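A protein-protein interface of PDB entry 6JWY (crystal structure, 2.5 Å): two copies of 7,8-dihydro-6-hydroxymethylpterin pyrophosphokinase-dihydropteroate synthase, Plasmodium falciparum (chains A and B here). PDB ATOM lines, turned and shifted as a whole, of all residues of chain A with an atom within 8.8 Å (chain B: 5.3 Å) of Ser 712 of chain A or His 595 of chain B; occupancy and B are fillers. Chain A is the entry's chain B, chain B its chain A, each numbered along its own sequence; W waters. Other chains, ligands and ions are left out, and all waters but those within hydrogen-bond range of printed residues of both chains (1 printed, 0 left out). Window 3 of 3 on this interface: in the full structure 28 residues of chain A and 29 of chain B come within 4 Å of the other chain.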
ATOM      1  N   VAL A 706      10.053   7.753  24.411  1.00  0.00           N
ATOM      2  CA  VAL A 706      10.634   8.142  23.135  1.00  0.00           C
ATOM      3  C   VAL A 706      10.639   9.668  23.045  1.00  0.00           C
ATOM      4  O   VAL A 706       9.651  10.316  23.392  1.00  0.00           O
ATOM      5  CB  VAL A 706       9.862   7.508  21.959  1.00  0.00           C
ATOM      6  CG1 VAL A 706      10.224   6.041  21.772  1.00  0.00           C
ATOM      7  CG2 VAL A 706       8.351   7.676  22.100  1.00  0.00           C
ATOM      8  N   ASP A 708      11.506  11.341  20.089  1.00  0.00           N
ATOM      9  CA  ASP A 708      11.077  11.646  18.736  1.00  0.00           C
ATOM     10  C   ASP A 708      10.401  10.409  18.156  1.00  0.00           C
ATOM     11  O   ASP A 708      11.067   9.437  17.811  1.00  0.00           O
ATOM     12  CB  ASP A 708      12.268  12.090  17.880  1.00  0.00           C
ATOM     13  CG  ASP A 708      11.906  12.639  16.507  1.00  0.00           C
ATOM     14  OD1 ASP A 708      10.696  12.715  16.192  1.00  0.00           O
ATOM     15  OD2 ASP A 708      12.846  12.996  15.761  1.00  0.00           O
ATOM     16  N   PRO A 709       9.058  10.406  18.042  1.00  0.00           N
ATOM     17  CA  PRO A 709       8.317   9.258  17.510  1.00  0.00           C
ATOM     18  C   PRO A 709       8.514   8.892  16.037  1.00  0.00           C
ATOM     19  O   PRO A 709       7.917   7.920  15.563  1.00  0.00           O
ATOM     20  CB  PRO A 709       6.843   9.652  17.716  1.00  0.00           C
ATOM     21  CG  PRO A 709       6.864  11.169  17.774  1.00  0.00           C
ATOM     22  CD  PRO A 709       8.169  11.500  18.472  1.00  0.00           C
ATOM     23  N   ASN A 710       9.317   9.671  15.298  1.00  0.00           N
ATOM     24  CA  ASN A 710       9.509   9.314  13.898  1.00  0.00           C
ATOM     25  C   ASN A 710      10.954   8.909  13.623  1.00  0.00           C
ATOM     26  O   ASN A 710      11.255   8.394  12.544  1.00  0.00           O
ATOM     27  CB  ASN A 710       8.752  10.197  12.885  1.00  0.00           C
ATOM     28  CG  ASN A 710       8.825  11.698  13.104  1.00  0.00           C
ATOM     29  OD1 ASN A 710       9.901  12.274  13.270  1.00  0.00           O
ATOM     30  ND2 ASN A 710       7.675  12.349  13.053  1.00  0.00           N
ATOM     31  N   SER A 711      11.812   9.067  14.641  1.00  0.00           N
ATOM     32  CA  SER A 711      13.239   8.802  14.513  1.00  0.00           C
ATOM     33  C   SER A 711      13.482   7.381  14.002  1.00  0.00           C
ATOM     34  O   SER A 711      14.422   7.121  13.260  1.00  0.00           O
ATOM     35  CB  SER A 711      13.977   9.075  15.804  1.00  0.00           C
ATOM     36  OG  SER A 711      13.633   8.122  16.802  1.00  0.00           O
ATOM     37  N   SER A 712      12.604   6.465  14.389  1.00  0.00           N
ATOM     38  CA  SER A 712      12.749   5.082  13.992  1.00  0.00           C
ATOM     39  C   SER A 712      12.727   4.933  12.465  1.00  0.00           C
ATOM     40  O   SER A 712      13.612   4.271  11.918  1.00  0.00           O
ATOM     41  CB  SER A 712      11.783   4.199  14.756  1.00  0.00           C
ATOM     42  OG  SER A 712      11.384   3.059  14.012  1.00  0.00           O
ATOM     43  N   SER A 713      11.778   5.581  11.764  1.00  0.00           N
ATOM     44  CA  SER A 713      11.687   5.420  10.310  1.00  0.00           C
ATOM     45  C   SER A 713      12.619   6.376   9.567  1.00  0.00           C
ATOM     46  O   SER A 713      13.167   6.029   8.518  1.00  0.00           O
ATOM     47  CB  SER A 713      10.278   5.539   9.801  1.00  0.00           C
ATOM     48  OG  SER A 713       9.731   6.785  10.196  1.00  0.00           O
ATOM     49  N   VAL A 714      12.794   7.582  10.124  1.00  0.00           N
ATOM     50  CA  VAL A 714      13.760   8.534   9.600  1.00  0.00           C
ATOM     51  C   VAL A 714      15.169   7.924   9.624  1.00  0.00           C
ATOM     52  O   VAL A 714      15.847   7.910   8.596  1.00  0.00           O
ATOM     53  CB  VAL A 714      13.684   9.879  10.350  1.00  0.00           C
ATOM     54  CG1 VAL A 714      14.799  10.811   9.918  1.00  0.00           C
ATOM     55  CG2 VAL A 714      12.334  10.552  10.156  1.00  0.00           C
ATOM     56  N   ASP A 715      15.600   7.405  10.787  1.00  0.00           N
ATOM     57  CA  ASP A 715      16.945   6.867  10.942  1.00  0.00           C
ATOM     58  C   ASP A 715      17.136   5.667  10.014  1.00  0.00           C
ATOM     59  O   ASP A 715      18.239   5.428   9.518  1.00  0.00           O
ATOM     60  CB  ASP A 715      17.315   6.604  12.407  1.00  0.00           C
ATOM     61  CG  ASP A 715      17.210   7.834  13.310  1.00  0.00           C
ATOM     62  OD1 ASP A 715      17.032   8.948  12.761  1.00  0.00           O
ATOM     63  OD2 ASP A 715      17.279   7.674  14.568  1.00  0.00           O
ATOM     64  N   LYS A 716      16.047   4.941   9.745  1.00  0.00           N
ATOM     65  CA  LYS A 716      16.138   3.810   8.842  1.00  0.00           C
ATOM     66  C   LYS A 716      16.435   4.316   7.432  1.00  0.00           C
ATOM     67  O   LYS A 716      17.334   3.806   6.754  1.00  0.00           O
ATOM     68  CB  LYS A 716      14.871   2.945   8.889  1.00  0.00           C
ATOM     69  CG  LYS A 716      14.966   1.705   8.014  1.00  0.00           C
ATOM     70  CD  LYS A 716      13.807   0.743   8.092  1.00  0.00           C
ATOM     71  CE  LYS A 716      14.042  -0.423   7.148  1.00  0.00           C
ATOM     72  NZ  LYS A 716      12.897  -1.368   7.105  1.00  0.00           N
ATOM     73  N   LEU A 717      15.679   5.342   7.011  1.00  0.00           N
ATOM     74  CA  LEU A 717      15.809   5.880   5.669  1.00  0.00           C
ATOM     75  C   LEU A 717      17.196   6.485   5.466  1.00  0.00           C
ATOM     76  O   LEU A 717      17.795   6.319   4.402  1.00  0.00           O
ATOM     77  CB  LEU A 717      14.691   6.893   5.404  1.00  0.00           C
ATOM     78  CG  LEU A 717      14.665   7.465   3.986  1.00  0.00           C
ATOM     79  CD1 LEU A 717      14.386   6.381   2.955  1.00  0.00           C
ATOM     80  CD2 LEU A 717      13.636   8.582   3.885  1.00  0.00           C
ATOM     81  N   ALA A 718      17.711   7.171   6.491  1.00  0.00           N
ATOM     82  CA  ALA A 718      19.040   7.742   6.392  1.00  0.00           C
ATOM     83  C   ALA A 718      20.068   6.644   6.121  1.00  0.00           C
ATOM     84  O   ALA A 718      20.936   6.812   5.269  1.00  0.00           O
ATOM     85  CB  ALA A 718      19.363   8.536   7.633  1.00  0.00           C
ATOM     86  N   ALA A 719      19.952   5.512   6.828  1.00  0.00           N
ATOM     87  CA  ALA A 719      20.902   4.412   6.700  1.00  0.00           C
ATOM     88  C   ALA A 719      20.877   3.856   5.278  1.00  0.00           C
ATOM     89  O   ALA A 719      21.926   3.515   4.731  1.00  0.00           O
ATOM     90  CB  ALA A 719      20.619   3.330   7.717  1.00  0.00           C
ATOM     91  N   TYR B 549      21.821   2.450  13.535  1.00  0.00           N
ATOM     92  CA  TYR B 549      22.122   1.784  12.269  1.00  0.00           C
ATOM     93  C   TYR B 549      23.629   1.644  12.101  1.00  0.00           C
ATOM     94  O   TYR B 549      24.080   0.732  11.410  1.00  0.00           O
ATOM     95  CB  TYR B 549      21.365   2.397  11.078  1.00  0.00           C
ATOM     96  CG  TYR B 549      19.883   2.114  11.109  1.00  0.00           C
ATOM     97  CD1 TYR B 549      19.056   2.868  11.935  1.00  0.00           C
ATOM     98  CD2 TYR B 549      19.315   1.065  10.389  1.00  0.00           C
ATOM     99  CE1 TYR B 549      17.704   2.603  12.045  1.00  0.00           C
ATOM    100  CE2 TYR B 549      17.958   0.776  10.487  1.00  0.00           C
ATOM    101  CZ  TYR B 549      17.161   1.548  11.329  1.00  0.00           C
ATOM    102  OH  TYR B 549      15.818   1.322  11.490  1.00  0.00           O
ATOM    103  N   GLN B 592      15.346   0.606  23.032  1.00  0.00           N
ATOM    104  CA  GLN B 592      14.101   1.070  22.435  1.00  0.00           C
ATOM    105  C   GLN B 592      13.964   0.611  20.986  1.00  0.00           C
ATOM    106  O   GLN B 592      12.856   0.354  20.534  1.00  0.00           O
ATOM    107  CB  GLN B 592      14.006   2.587  22.456  1.00  0.00           C
ATOM    108  CG  GLN B 592      14.115   3.158  23.855  1.00  0.00           C
ATOM    109  CD  GLN B 592      14.084   4.660  23.855  1.00  0.00           C
ATOM    110  OE1 GLN B 592      14.305   5.302  22.834  1.00  0.00           O
ATOM    111  NE2 GLN B 592      13.803   5.235  25.013  1.00  0.00           N
ATOM    112  N   ASN B 593      15.076   0.516  20.246  1.00  0.00           N
ATOM    113  CA  ASN B 593      14.994   0.198  18.830  1.00  0.00           C
ATOM    114  C   ASN B 593      15.514  -1.205  18.552  1.00  0.00           C
ATOM    115  O   ASN B 593      16.031  -1.460  17.474  1.00  0.00           O
ATOM    116  CB  ASN B 593      15.851   1.134  17.977  1.00  0.00           C
ATOM    117  CG  ASN B 593      15.385   2.565  18.047  1.00  0.00           C
ATOM    118  OD1 ASN B 593      14.602   3.001  17.198  1.00  0.00           O
ATOM    119  ND2 ASN B 593      15.847   3.280  19.063  1.00  0.00           N
ATOM    120  N   ILE B 594      15.368  -2.112  19.513  1.00  0.00           N
ATOM    121  CA  ILE B 594      15.846  -3.472  19.317  1.00  0.00           C
ATOM    122  C   ILE B 594      15.129  -4.157  18.141  1.00  0.00           C
ATOM    123  O   ILE B 594      15.614  -5.175  17.651  1.00  0.00           O
ATOM    124  CB  ILE B 594      15.764  -4.279  20.631  1.00  0.00           C
ATOM    125  CG1 ILE B 594      16.817  -5.386  20.688  1.00  0.00           C
ATOM    126  CG2 ILE B 594      14.375  -4.833  20.846  1.00  0.00           C
ATOM    127  CD1 ILE B 594      18.232  -4.882  20.835  1.00  0.00           C
ATOM    128  N   HIS B 595      14.009  -3.587  17.664  1.00  0.00           N
ATOM    129  CA  HIS B 595      13.192  -4.227  16.639  1.00  0.00           C
ATOM    130  C   HIS B 595      13.989  -4.444  15.356  1.00  0.00           C
ATOM    131  O   HIS B 595      13.678  -5.291  14.518  1.00  0.00           O
ATOM    132  CB  HIS B 595      11.924  -3.412  16.351  1.00  0.00           C
ATOM    133  CG  HIS B 595      12.201  -2.074  15.773  1.00  0.00           C
ATOM    134  ND1 HIS B 595      12.461  -0.985  16.571  1.00  0.00           N
ATOM    135  CD2 HIS B 595      12.302  -1.656  14.492  1.00  0.00           C
ATOM    136  CE1 HIS B 595      12.731   0.066  15.813  1.00  0.00           C
ATOM    137  NE2 HIS B 595      12.625  -0.323  14.523  1.00  0.00           N
ATOM    138  N   VAL B 596      15.013  -3.624  15.219  1.00  0.00           N
ATOM    139  CA  VAL B 596      15.906  -3.600  14.080  1.00  0.00           C
ATOM    140  C   VAL B 596      16.590  -4.964  13.892  1.00  0.00           C
ATOM    141  O   VAL B 596      17.069  -5.262  12.790  1.00  0.00           O
ATOM    142  CB  VAL B 596      16.847  -2.414  14.335  1.00  0.00           C
ATOM    143  CG1 VAL B 596      18.328  -2.711  14.258  1.00  0.00           C
ATOM    144  CG2 VAL B 596      16.403  -1.160  13.612  1.00  0.00           C
ATOM    145  N   TYR B 597      16.570  -5.807  14.938  1.00  0.00           N
ATOM    146  CA  TYR B 597      17.143  -7.141  14.835  1.00  0.00           C
ATOM    147  C   TYR B 597      16.073  -8.236  14.718  1.00  0.00           C
ATOM    148  O   TYR B 597      16.368  -9.390  15.050  1.00  0.00           O
ATOM    149  CB  TYR B 597      18.108  -7.419  15.993  1.00  0.00           C
ATOM    150  CG  TYR B 597      19.258  -6.448  16.053  1.00  0.00           C
ATOM    151  CD1 TYR B 597      19.152  -5.286  16.798  1.00  0.00           C
ATOM    152  CD2 TYR B 597      20.411  -6.647  15.301  1.00  0.00           C
ATOM    153  CE1 TYR B 597      20.176  -4.348  16.812  1.00  0.00           C
ATOM    154  CE2 TYR B 597      21.446  -5.728  15.313  1.00  0.00           C
ATOM    155  CZ  TYR B 597      21.316  -4.575  16.064  1.00  0.00           C
ATOM    156  OH  TYR B 597      22.302  -3.639  16.089  1.00  0.00           O
ATOM    157  N   ASP B 598      14.870  -7.898  14.204  1.00  0.00           N
ATOM    158  CA  ASP B 598      13.780  -8.860  14.085  1.00  0.00           C
ATOM    159  C   ASP B 598      14.129  -9.950  13.074  1.00  0.00           C
ATOM    160  O   ASP B 598      13.540 -11.030  13.105  1.00  0.00           O
ATOM    161  CB  ASP B 598      12.447  -8.245  13.632  1.00  0.00           C
ATOM    162  CG  ASP B 598      11.686  -7.391  14.642  1.00  0.00           C
ATOM    163  OD1 ASP B 598      12.069  -7.369  15.866  1.00  0.00           O
ATOM    164  OD2 ASP B 598      10.696  -6.738  14.207  1.00  0.00           O
ATOM    165  N   GLU B 599      15.054  -9.688  12.157  1.00  0.00           N
ATOM    166  CA  GLU B 599      15.335 -10.734  11.190  1.00  0.00           C
ATOM    167  C   GLU B 599      16.511 -11.607  11.648  1.00  0.00           C
ATOM    168  O   GLU B 599      16.895 -12.505  10.894  1.00  0.00           O
ATOM    169  CB  GLU B 599      15.709 -10.152   9.822  1.00  0.00           C
ATOM    170  CG  GLU B 599      14.562  -9.563   9.024  1.00  0.00           C
ATOM    171  CD  GLU B 599      13.360 -10.469   8.840  1.00  0.00           C
ATOM    172  OE1 GLU B 599      13.497 -11.508   8.153  1.00  0.00           O
ATOM    173  OE2 GLU B 599      12.291 -10.137   9.407  1.00  0.00           O
ATOM    174  N   LYS B 680       9.902  -8.609  22.940  1.00  0.00           N
ATOM    175  CA  LYS B 680      10.546  -8.285  21.684  1.00  0.00           C
ATOM    176  C   LYS B 680      11.137  -9.552  21.076  1.00  0.00           C
ATOM    177  O   LYS B 680      11.675  -9.513  19.977  1.00  0.00           O
ATOM    178  CB  LYS B 680      11.550  -7.145  21.860  1.00  0.00           C
ATOM    179  CG  LYS B 680      10.900  -5.794  22.122  1.00  0.00           C
ATOM    180  CD  LYS B 680      10.326  -5.225  20.865  1.00  0.00           C
ATOM    181  CE  LYS B 680       9.720  -3.853  21.062  1.00  0.00           C
ATOM    182  NZ  LYS B 680       9.225  -3.321  19.766  1.00  0.00           N
HETATM  183  O   HOH W   1      15.562   3.166  14.518  1.00  0.00           O
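Of chain B, only Tyr 549, Asn 593 and His 595 come within 4 Å of Ser 712 of chain A. His 595 of chain B touches just one residue of chain A: Ser 712 (3.6 Å). Of the printed residues of chain A, Asn 593 of chain B touches Ser 712. Of the printed residues of chain B, Asp 715 of chain A touches Tyr 549 (3.6 Å). Of the printed residues of chain B, Lys 716 of chain A touches Tyr 549. Printed residues of chain B within 4 Å of Ala 719 of chain A: Tyr 549 (3.6 Å). Tyr 597 of chain B touches none of the printed residues of chain A. Asn 710 of chain A touches none of the printed residues of chain B. The nearest residue of chain A that does not touch His 595 of chain B is Ser 713 of chain A (6.6 Å). The nearest printed residue of chain B that does not touch Asp 715 of chain A is Asn 593 of chain B (6.0 Å).
Tyr 549 of chain B touches Ser 712 of chain A (OH to O, 3.7 Å). Ser 712 of chain A touches Asn 593 of chain B. NE2 of His 595 of chain B touches OG of Ser 712 of chain A, 3.6 Å away. CD1 of Tyr 549 of chain B touches O of Asp 715 of chain A, 3.6 Å away. Lys 716 of chain A touches Tyr 549 of chain B. CB of Tyr 549 of chain B touches CB of Ala 719 of chain A, at 3.6 Å.
No position is printed for both chains. Of the 6 pairs that touch across the chains among the printed residues, none has its exchanged pair printed and touching as well.
Of the 13 printed residues of chain A, 4 touch a printed residue of chain B. Hydrophobic or aromatic side chains of chain A that line the printed part of chain B: Ala 719. Along chain A the printed residues that touch a printed residue of chain B span positions 712 to 719. Hydrophobic or aromatic side chains of chain B within 4 Å of the printed part of chain A: Tyr 549 and His 595. Among the printed residues, no Asp or Glu carboxylate lies within 4 Å of a Lys or Arg side-chain nitrogen of the other chain.
Water W1 lies within hydrogen-bond range of the side-chain amide oxygen (OD1) of Asn 593 of chain B (2.9 Å) and the backbone carbonyl oxygen (O) of Ser 712 of chain A (3.4 Å).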
